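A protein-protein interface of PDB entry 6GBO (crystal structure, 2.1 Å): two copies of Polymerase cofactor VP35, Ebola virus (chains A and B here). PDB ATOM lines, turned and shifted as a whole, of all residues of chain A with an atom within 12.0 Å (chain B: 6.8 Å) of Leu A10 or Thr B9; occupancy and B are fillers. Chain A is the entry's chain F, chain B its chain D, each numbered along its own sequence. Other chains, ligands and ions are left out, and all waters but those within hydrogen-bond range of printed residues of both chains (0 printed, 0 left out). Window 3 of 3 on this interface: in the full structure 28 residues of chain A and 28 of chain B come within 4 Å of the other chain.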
ATOM      1  N   MET A   1      16.586  -3.643 -10.354  1.00  0.00           N
ATOM      2  CA  MET A   1      15.163  -3.403  -9.969  1.00  0.00           C
ATOM      3  C   MET A   1      14.361  -4.703  -9.812  1.00  0.00           C
ATOM      4  O   MET A   1      13.168  -4.729 -10.099  1.00  0.00           O
ATOM      5  CB  MET A   1      14.492  -2.485 -10.993  1.00  0.00           C
ATOM      6  N   SER A   2      15.012  -5.775  -9.359  1.00  0.00           N
ATOM      7  CA  SER A   2      14.322  -7.028  -9.025  1.00  0.00           C
ATOM      8  C   SER A   2      13.976  -7.028  -7.541  1.00  0.00           C
ATOM      9  O   SER A   2      14.572  -6.281  -6.769  1.00  0.00           O
ATOM     10  CB  SER A   2      15.193  -8.243  -9.359  1.00  0.00           C
ATOM     11  OG  SER A   2      16.580  -7.864  -9.465  1.00  0.00           O
ATOM     12  N   PHE A   3      13.019  -7.861  -7.136  1.00  0.00           N
ATOM     13  CA  PHE A   3      12.640  -7.925  -5.727  1.00  0.00           C
ATOM     14  C   PHE A   3      13.730  -8.605  -4.898  1.00  0.00           C
ATOM     15  O   PHE A   3      14.006  -8.178  -3.772  1.00  0.00           O
ATOM     16  CB  PHE A   3      11.293  -8.622  -5.523  1.00  0.00           C
ATOM     17  CG  PHE A   3      10.678  -8.352  -4.172  1.00  0.00           C
ATOM     18  CD1 PHE A   3      10.111  -7.112  -3.883  1.00  0.00           C
ATOM     19  CD2 PHE A   3      10.681  -9.324  -3.182  1.00  0.00           C
ATOM     20  CE1 PHE A   3       9.554  -6.854  -2.636  1.00  0.00           C
ATOM     21  CE2 PHE A   3      10.128  -9.069  -1.934  1.00  0.00           C
ATOM     22  CZ  PHE A   3       9.560  -7.834  -1.661  1.00  0.00           C
ATOM     23  N   GLU A   4      14.352  -9.650  -5.444  1.00  0.00           N
ATOM     24  CA  GLU A   4      15.519 -10.251  -4.789  1.00  0.00           C
ATOM     25  C   GLU A   4      16.656  -9.256  -4.657  1.00  0.00           C
ATOM     26  O   GLU A   4      17.392  -9.299  -3.681  1.00  0.00           O
ATOM     27  CB  GLU A   4      16.021 -11.487  -5.527  1.00  0.00           C
ATOM     28  CG  GLU A   4      15.587 -12.781  -4.873  1.00  0.00           C
ATOM     29  CD  GLU A   4      15.982 -13.991  -5.689  1.00  0.00           C
ATOM     30  OE1 GLU A   4      17.124 -14.474  -5.529  1.00  0.00           O
ATOM     31  OE2 GLU A   4      15.146 -14.452  -6.490  1.00  0.00           O
ATOM     32  N   GLU A   5      16.804  -8.386  -5.653  1.00  0.00           N
ATOM     33  CA  GLU A   5      17.796  -7.312  -5.608  1.00  0.00           C
ATOM     34  C   GLU A   5      17.485  -6.295  -4.499  1.00  0.00           C
ATOM     35  O   GLU A   5      18.377  -5.909  -3.733  1.00  0.00           O
ATOM     36  CB  GLU A   5      17.900  -6.618  -6.978  1.00  0.00           C
ATOM     37  CG  GLU A   5      18.589  -5.250  -6.973  1.00  0.00           C
ATOM     38  CD  GLU A   5      17.623  -4.091  -6.758  1.00  0.00           C
ATOM     39  OE1 GLU A   5      16.621  -4.011  -7.501  1.00  0.00           O
ATOM     40  OE2 GLU A   5      17.868  -3.256  -5.862  1.00  0.00           O
ATOM     41  N   VAL A   6      16.230  -5.859  -4.423  1.00  0.00           N
ATOM     42  CA  VAL A   6      15.818  -4.890  -3.410  1.00  0.00           C
ATOM     43  C   VAL A   6      16.007  -5.453  -2.003  1.00  0.00           C
ATOM     44  O   VAL A   6      16.514  -4.760  -1.120  1.00  0.00           O
ATOM     45  CB  VAL A   6      14.358  -4.441  -3.610  1.00  0.00           C
ATOM     46  CG1 VAL A   6      13.840  -3.690  -2.390  1.00  0.00           C
ATOM     47  CG2 VAL A   6      14.249  -3.563  -4.847  1.00  0.00           C
ATOM     48  N   VAL A   7      15.617  -6.710  -1.808  1.00  0.00           N
ATOM     49  CA  VAL A   7      15.700  -7.347  -0.492  1.00  0.00           C
ATOM     50  C   VAL A   7      17.154  -7.504  -0.017  1.00  0.00           C
ATOM     51  O   VAL A   7      17.461  -7.199   1.139  1.00  0.00           O
ATOM     52  CB  VAL A   7      14.963  -8.710  -0.474  1.00  0.00           C
ATOM     53  CG1 VAL A   7      15.217  -9.464   0.826  1.00  0.00           C
ATOM     54  CG2 VAL A   7      13.462  -8.507  -0.677  1.00  0.00           C
ATOM     55  N   GLN A   8      18.042  -7.968  -0.898  1.00  0.00           N
ATOM     56  CA  GLN A   8      19.462  -8.157  -0.540  1.00  0.00           C
ATOM     57  C   GLN A   8      20.182  -6.845  -0.232  1.00  0.00           C
ATOM     58  O   GLN A   8      21.036  -6.793   0.657  1.00  0.00           O
ATOM     59  CB  GLN A   8      20.217  -8.894  -1.650  1.00  0.00           C
ATOM     60  CG  GLN A   8      19.901 -10.376  -1.733  1.00  0.00           C
ATOM     61  CD  GLN A   8      20.575 -11.052  -2.913  1.00  0.00           C
ATOM     62  OE1 GLN A   8      21.416 -10.459  -3.591  1.00  0.00           O
ATOM     63  NE2 GLN A   8      20.207 -12.301  -3.166  1.00  0.00           N
ATOM     64  N   THR A   9      19.843  -5.797  -0.977  1.00  0.00           N
ATOM     65  CA  THR A   9      20.441  -4.476  -0.772  1.00  0.00           C
ATOM     66  C   THR A   9      19.924  -3.837   0.520  1.00  0.00           C
ATOM     67  O   THR A   9      20.668  -3.144   1.222  1.00  0.00           O
ATOM     68  CB  THR A   9      20.159  -3.560  -1.979  1.00  0.00           C
ATOM     69  OG1 THR A   9      20.680  -4.172  -3.169  1.00  0.00           O
ATOM     70  CG2 THR A   9      20.788  -2.189  -1.804  1.00  0.00           C
ATOM     71  N   LEU A  10      18.649  -4.079   0.827  1.00  0.00           N
ATOM     72  CA  LEU A  10      18.042  -3.617   2.071  1.00  0.00           C
ATOM     73  C   LEU A  10      18.640  -4.324   3.289  1.00  0.00           C
ATOM     74  O   LEU A  10      18.862  -3.694   4.331  1.00  0.00           O
ATOM     75  CB  LEU A  10      16.530  -3.829   2.039  1.00  0.00           C
ATOM     76  CG  LEU A  10      15.737  -3.382   3.268  1.00  0.00           C
ATOM     77  CD1 LEU A  10      15.954  -1.901   3.550  1.00  0.00           C
ATOM     78  CD2 LEU A  10      14.257  -3.681   3.091  1.00  0.00           C
ATOM     79  N   ALA A  11      18.893  -5.626   3.163  1.00  0.00           N
ATOM     80  CA  ALA A  11      19.563  -6.379   4.219  1.00  0.00           C
ATOM     81  C   ALA A  11      20.998  -5.884   4.413  1.00  0.00           C
ATOM     82  O   ALA A  11      21.476  -5.803   5.545  1.00  0.00           O
ATOM     83  CB  ALA A  11      19.550  -7.867   3.911  1.00  0.00           C
ATOM     84  N   SER A  12      21.669  -5.548   3.309  1.00  0.00           N
ATOM     85  CA  SER A  12      23.017  -4.972   3.351  1.00  0.00           C
ATOM     86  C   SER A  12      23.040  -3.644   4.103  1.00  0.00           C
ATOM     87  O   SER A  12      23.815  -3.475   5.040  1.00  0.00           O
ATOM     88  CB  SER A  12      23.573  -4.756   1.938  1.00  0.00           C
ATOM     89  OG  SER A  12      23.899  -5.984   1.321  1.00  0.00           O
ATOM     90  N   LEU A  13      22.195  -2.706   3.674  1.00  0.00           N
ATOM     91  CA  LEU A  13      22.051  -1.412   4.351  1.00  0.00           C
ATOM     92  C   LEU A  13      21.767  -1.563   5.840  1.00  0.00           C
ATOM     93  O   LEU A  13      22.393  -0.899   6.665  1.00  0.00           O
ATOM     94  CB  LEU A  13      20.917  -0.573   3.736  1.00  0.00           C
ATOM     95  CG  LEU A  13      21.253   0.608   2.817  1.00  0.00           C
ATOM     96  CD1 LEU A  13      20.059   1.547   2.742  1.00  0.00           C
ATOM     97  CD2 LEU A  13      22.471   1.384   3.281  1.00  0.00           C
ATOM     98  N   ALA A  14      20.805  -2.420   6.167  1.00  0.00           N
ATOM     99  CA  ALA A  14      20.390  -2.634   7.547  1.00  0.00           C
ATOM    100  C   ALA A  14      21.585  -2.927   8.436  1.00  0.00           C
ATOM    101  O   ALA A  14      21.687  -2.385   9.531  1.00  0.00           O
ATOM    102  CB  ALA A  14      19.391  -3.779   7.632  1.00  0.00           C
ATOM    103  N   THR A  15      22.485  -3.781   7.950  1.00  0.00           N
ATOM    104  CA  THR A  15      23.637  -4.218   8.728  1.00  0.00           C
ATOM    105  C   THR A  15      24.679  -3.112   8.810  1.00  0.00           C
ATOM    106  O   THR A  15      25.320  -2.957   9.840  1.00  0.00           O
ATOM    107  CB  THR A  15      24.284  -5.505   8.161  1.00  0.00           C
ATOM    108  OG1 THR A  15      24.784  -5.262   6.838  1.00  0.00           O
ATOM    109  CG2 THR A  15      23.277  -6.673   8.134  1.00  0.00           C
ATOM    110  N   VAL A  16      24.840  -2.349   7.732  1.00  0.00           N
ATOM    111  CA  VAL A  16      25.757  -1.209   7.733  1.00  0.00           C
ATOM    112  C   VAL A  16      25.290  -0.143   8.722  1.00  0.00           C
ATOM    113  O   VAL A  16      26.096   0.425   9.452  1.00  0.00           O
ATOM    114  CB  VAL A  16      25.919  -0.603   6.326  1.00  0.00           C
ATOM    115  CG1 VAL A  16      26.624   0.746   6.387  1.00  0.00           C
ATOM    116  CG2 VAL A  16      26.699  -1.561   5.446  1.00  0.00           C
ATOM    117  N   VAL A  17      23.990   0.115   8.746  1.00  0.00           N
ATOM    118  CA  VAL A  17      23.409   1.024   9.722  1.00  0.00           C
ATOM    119  C   VAL A  17      23.627   0.517  11.140  1.00  0.00           C
ATOM    120  O   VAL A  17      24.019   1.284  12.012  1.00  0.00           O
ATOM    121  CB  VAL A  17      21.910   1.252   9.465  1.00  0.00           C
ATOM    122  CG1 VAL A  17      21.216   1.854  10.680  1.00  0.00           C
ATOM    123  CG2 VAL A  17      21.741   2.156   8.256  1.00  0.00           C
ATOM    124  N   GLN A  18      23.352  -0.765  11.367  1.00  0.00           N
ATOM    125  CA  GLN A  18      23.660  -1.407  12.653  1.00  0.00           C
ATOM    126  C   GLN A  18      25.133  -1.242  13.018  1.00  0.00           C
ATOM    127  O   GLN A  18      25.457  -0.942  14.173  1.00  0.00           O
ATOM    128  CB  GLN A  18      23.265  -2.891  12.634  1.00  0.00           C
ATOM    129  CG  GLN A  18      21.775  -3.116  12.881  1.00  0.00           C
ATOM    130  CD  GLN A  18      21.178  -4.293  12.107  1.00  0.00           C
ATOM    131  OE1 GLN A  18      21.790  -5.362  11.982  1.00  0.00           O
ATOM    132  NE2 GLN A  18      19.963  -4.101  11.595  1.00  0.00           N
ATOM    133  N   GLN A  19      26.019  -1.429  12.039  1.00  0.00           N
ATOM    134  CA  GLN A  19      27.464  -1.253  12.261  1.00  0.00           C
ATOM    135  C   GLN A  19      27.779   0.165  12.748  1.00  0.00           C
ATOM    136  O   GLN A  19      28.548   0.344  13.687  1.00  0.00           O
ATOM    137  CB  GLN A  19      28.263  -1.545  10.985  1.00  0.00           C
ATOM    138  CG  GLN A  19      28.614  -3.020  10.774  1.00  0.00           C
ATOM    139  CD  GLN A  19      28.949  -3.379   9.323  1.00  0.00           C
ATOM    140  OE1 GLN A  19      29.335  -2.527   8.515  1.00  0.00           O
ATOM    141  NE2 GLN A  19      28.794  -4.651   8.989  1.00  0.00           N
ATOM    142  N   GLN A  20      27.178   1.161  12.101  1.00  0.00           N
ATOM    143  CA  GLN A  20      27.433   2.559  12.419  1.00  0.00           C
ATOM    144  C   GLN A  20      26.969   2.928  13.828  1.00  0.00           C
ATOM    145  O   GLN A  20      27.624   3.718  14.513  1.00  0.00           O
ATOM    146  CB  GLN A  20      26.809   3.479  11.366  1.00  0.00           C
ATOM    147  CG  GLN A  20      27.600   3.500  10.055  1.00  0.00           C
ATOM    148  CD  GLN A  20      26.944   4.345   8.956  1.00  0.00           C
ATOM    149  OE1 GLN A  20      25.719   4.346   8.794  1.00  0.00           O
ATOM    150  NE2 GLN A  20      27.763   5.056   8.186  1.00  0.00           N
ATOM    151  N   PHE B   3       6.290  -6.928  -0.059  1.00  0.00           N
ATOM    152  CA  PHE B   3       6.500  -5.552  -0.502  1.00  0.00           C
ATOM    153  C   PHE B   3       6.138  -4.562   0.597  1.00  0.00           C
ATOM    154  O   PHE B   3       6.879  -3.618   0.863  1.00  0.00           O
ATOM    155  CB  PHE B   3       5.651  -5.257  -1.734  1.00  0.00           C
ATOM    156  CG  PHE B   3       5.948  -3.931  -2.362  1.00  0.00           C
ATOM    157  CD1 PHE B   3       6.956  -3.811  -3.309  1.00  0.00           C
ATOM    158  CD2 PHE B   3       5.231  -2.801  -1.999  1.00  0.00           C
ATOM    159  CE1 PHE B   3       7.241  -2.587  -3.889  1.00  0.00           C
ATOM    160  CE2 PHE B   3       5.514  -1.573  -2.573  1.00  0.00           C
ATOM    161  CZ  PHE B   3       6.520  -1.466  -3.520  1.00  0.00           C
ATOM    162  N   GLU B   4       4.987  -4.786   1.221  1.00  0.00           N
ATOM    163  CA  GLU B   4       4.538  -4.000   2.369  1.00  0.00           C
ATOM    164  C   GLU B   4       5.633  -3.903   3.435  1.00  0.00           C
ATOM    165  O   GLU B   4       5.905  -2.820   3.958  1.00  0.00           O
ATOM    166  CB  GLU B   4       3.269  -4.642   2.960  1.00  0.00           C
ATOM    167  CG  GLU B   4       2.723  -3.995   4.232  1.00  0.00           C
ATOM    168  CD  GLU B   4       2.219  -2.576   4.019  1.00  0.00           C
ATOM    169  OE1 GLU B   4       1.446  -2.349   3.060  1.00  0.00           O
ATOM    170  OE2 GLU B   4       2.587  -1.693   4.823  1.00  0.00           O
ATOM    171  N   GLU B   5       6.243  -5.048   3.738  1.00  0.00           N
ATOM    172  CA  GLU B   5       7.323  -5.158   4.722  1.00  0.00           C
ATOM    173  C   GLU B   5       8.593  -4.407   4.309  1.00  0.00           C
ATOM    174  O   GLU B   5       9.301  -3.869   5.159  1.00  0.00           O
ATOM    175  CB  GLU B   5       7.645  -6.638   4.949  1.00  0.00           C
ATOM    176  CG  GLU B   5       8.824  -6.941   5.863  1.00  0.00           C
ATOM    177  CD  GLU B   5       9.306  -8.374   5.727  1.00  0.00           C
ATOM    178  OE1 GLU B   5       8.632  -9.189   5.055  1.00  0.00           O
ATOM    179  OE2 GLU B   5      10.372  -8.687   6.289  1.00  0.00           O
ATOM    180  N   VAL B   6       8.893  -4.395   3.012  1.00  0.00           N
ATOM    181  CA  VAL B   6      10.042  -3.649   2.499  1.00  0.00           C
ATOM    182  C   VAL B   6       9.838  -2.132   2.641  1.00  0.00           C
ATOM    183  O   VAL B   6      10.774  -1.415   3.005  1.00  0.00           O
ATOM    184  CB  VAL B   6      10.347  -4.038   1.036  1.00  0.00           C
ATOM    185  CG1 VAL B   6      11.293  -3.050   0.376  1.00  0.00           C
ATOM    186  CG2 VAL B   6      10.929  -5.442   0.984  1.00  0.00           C
ATOM    187  N   VAL B   7       8.627  -1.648   2.371  1.00  0.00           N
ATOM    188  CA  VAL B   7       8.322  -0.220   2.502  1.00  0.00           C
ATOM    189  C   VAL B   7       8.453   0.232   3.955  1.00  0.00           C
ATOM    190  O   VAL B   7       9.097   1.246   4.246  1.00  0.00           O
ATOM    191  CB  VAL B   7       6.896   0.124   2.004  1.00  0.00           C
ATOM    192  CG1 VAL B   7       6.524   1.567   2.354  1.00  0.00           C
ATOM    193  CG2 VAL B   7       6.784  -0.108   0.504  1.00  0.00           C
ATOM    194  N   GLN B   8       7.835  -0.521   4.860  1.00  0.00           N
ATOM    195  CA  GLN B   8       7.872  -0.186   6.281  1.00  0.00           C
ATOM    196  C   GLN B   8       9.280  -0.267   6.846  1.00  0.00           C
ATOM    197  O   GLN B   8       9.635   0.502   7.747  1.00  0.00           O
ATOM    198  CB  GLN B   8       6.936  -1.087   7.091  1.00  0.00           C
ATOM    199  CG  GLN B   8       5.516  -0.557   7.178  1.00  0.00           C
ATOM    200  CD  GLN B   8       4.536  -1.592   7.706  1.00  0.00           C
ATOM    201  OE1 GLN B   8       4.937  -2.626   8.244  1.00  0.00           O
ATOM    202  NE2 GLN B   8       3.244  -1.317   7.556  1.00  0.00           N
ATOM    203  N   THR B   9      10.077  -1.202   6.330  1.00  0.00           N
ATOM    204  CA  THR B   9      11.470  -1.308   6.744  1.00  0.00           C
ATOM    205  C   THR B   9      12.259  -0.089   6.285  1.00  0.00           C
ATOM    206  O   THR B   9      13.044   0.458   7.062  1.00  0.00           O
ATOM    207  CB  THR B   9      12.141  -2.593   6.225  1.00  0.00           C
ATOM    208  OG1 THR B   9      11.426  -3.729   6.716  1.00  0.00           O
ATOM    209  CG2 THR B   9      13.591  -2.683   6.706  1.00  0.00           C
ATOM    210  N   LEU B  10      12.046   0.349   5.044  1.00  0.00           N
ATOM    211  CA  LEU B  10      12.740   1.538   4.536  1.00  0.00           C
ATOM    212  C   LEU B  10      12.468   2.808   5.362  1.00  0.00           C
ATOM    213  O   LEU B  10      13.395   3.574   5.633  1.00  0.00           O
ATOM    214  CB  LEU B  10      12.419   1.804   3.063  1.00  0.00           C
ATOM    215  CG  LEU B  10      13.311   1.130   2.022  1.00  0.00           C
ATOM    216  CD1 LEU B  10      12.739   1.382   0.638  1.00  0.00           C
ATOM    217  CD2 LEU B  10      14.745   1.626   2.095  1.00  0.00           C
ATOM    218  N   ALA B  11      11.207   3.020   5.748  1.00  0.00           N
ATOM    219  CA  ALA B  11      10.807   4.198   6.533  1.00  0.00           C
ATOM    220  C   ALA B  11      11.386   4.172   7.950  1.00  0.00           C
ATOM    221  O   ALA B  11      11.813   5.195   8.477  1.00  0.00           O
ATOM    222  CB  ALA B  11       9.290   4.301   6.594  1.00  0.00           C
ATOM    223  N   SER B  12      11.387   2.988   8.553  1.00  0.00           N
ATOM    224  CA  SER B  12      11.943   2.776   9.876  1.00  0.00           C
ATOM    225  C   SER B  12      13.460   2.953   9.847  1.00  0.00           C
ATOM    226  O   SER B  12      14.043   3.572  10.739  1.00  0.00           O
ATOM    227  CB  SER B  12      11.573   1.370  10.364  1.00  0.00           C
ATOM    228  OG  SER B  12      12.081   1.120  11.662  1.00  0.00           O
ATOM    229  N   LEU B  13      14.087   2.418   8.807  1.00  0.00           N
ATOM    230  CA  LEU B  13      15.522   2.559   8.602  1.00  0.00           C
ATOM    231  C   LEU B  13      15.904   4.012   8.320  1.00  0.00           C
ATOM    232  O   LEU B  13      16.992   4.456   8.686  1.00  0.00           O
ATOM    233  CB  LEU B  13      15.986   1.666   7.446  1.00  0.00           C
ATOM    234  CG  LEU B  13      17.368   1.030   7.551  1.00  0.00           C
ATOM    235  CD1 LEU B  13      17.473   0.200   8.827  1.00  0.00           C
ATOM    236  CD2 LEU B  13      17.658   0.166   6.330  1.00  0.00           C
ATOM    237  N   ALA B  14      15.013   4.748   7.664  1.00  0.00           N
ATOM    238  CA  ALA B  14      15.247   6.165   7.404  1.00  0.00           C
ATOM    239  C   ALA B  14      15.301   6.932   8.716  1.00  0.00           C
ATOM    240  O   ALA B  14      16.182   7.750   8.911  1.00  0.00           O
ATOM    241  CB  ALA B  14      14.165   6.734   6.503  1.00  0.00           C
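The side-chain hydroxyl (OG1) of Thr B9 is in hydrogen-bond range of the backbone carbonyl oxygen (O) of Glu B5.
Among the printed residues, pairs that only touch across the chains: Phe A3 with Phe B3 (3.8 Å), Phe A3 with Val B6 (3.8 Å), Val A6 with Val B6 (3.8 Å), Leu A10 with Thr B9 (3.8 Å) and Leu A10 with Leu B13 (3.9 Å).
Of the printed residues of chain B, Phe A3 touches Phe B3 (3.8 Å) and Val B6 (3.8 Å). Printed residues of chain B within 4 Å of Val A6: Val B6 (3.8 Å). Printed residues of chain B within 4 Å of Leu A10: Thr B9 (3.8 Å) and Leu B13 (3.9 Å). Leu A13 touches none of the printed residues of chain B. Ala A14 touches none of the printed residues of chain B. Of the printed residues of chain A, Phe B3 touches Phe A3. No residue of chain A comes within 4 Å of Glu B5. Printed residues of chain A within 4 Å of Val B6: Phe A3 and Val A6. Thr B9 touches one residue of chain A. Ala B11 touches none of the printed residues of chain A. No residue of chain A comes within 4 Å of Ser B12. Leu B13 touches just one residue of chain A: Leu A10 (3.9 Å).
Printed residues of chain A that touch a printed residue of chain B: Phe A3, Val A6 and Leu A10. Hydrophobic or aromatic side chains of chain A that line the printed part of chain B: Phe A3, Val A6 and Leu A10. Of the 12 printed residues of chain B, 4 touch a printed residue of chain A. Hydrophobic or aromatic side chains of chain B within 4 Å of the printed part of chain A: Val B6 and Leu B13. Among the printed residues, 5 pairs touch across the chains. Among the printed residues, no Asp or Glu carboxylate lies within 4 Å of a Lys or Arg side-chain nitrogen of the other chain.
Phe A3 touches Val B6, but with the chains exchanged Val A6 does not touch Phe B3 (6.9 Å). Val B6 touches its own counterpart, Val A6. Leu A10 touches Thr B9, but with the chains exchanged Thr A9 does not touch Leu B10 (7.7 Å). Leu A10 touches Leu B13, but with the chains exchanged Leu A13 does not touch Leu B10 (5.4 Å).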
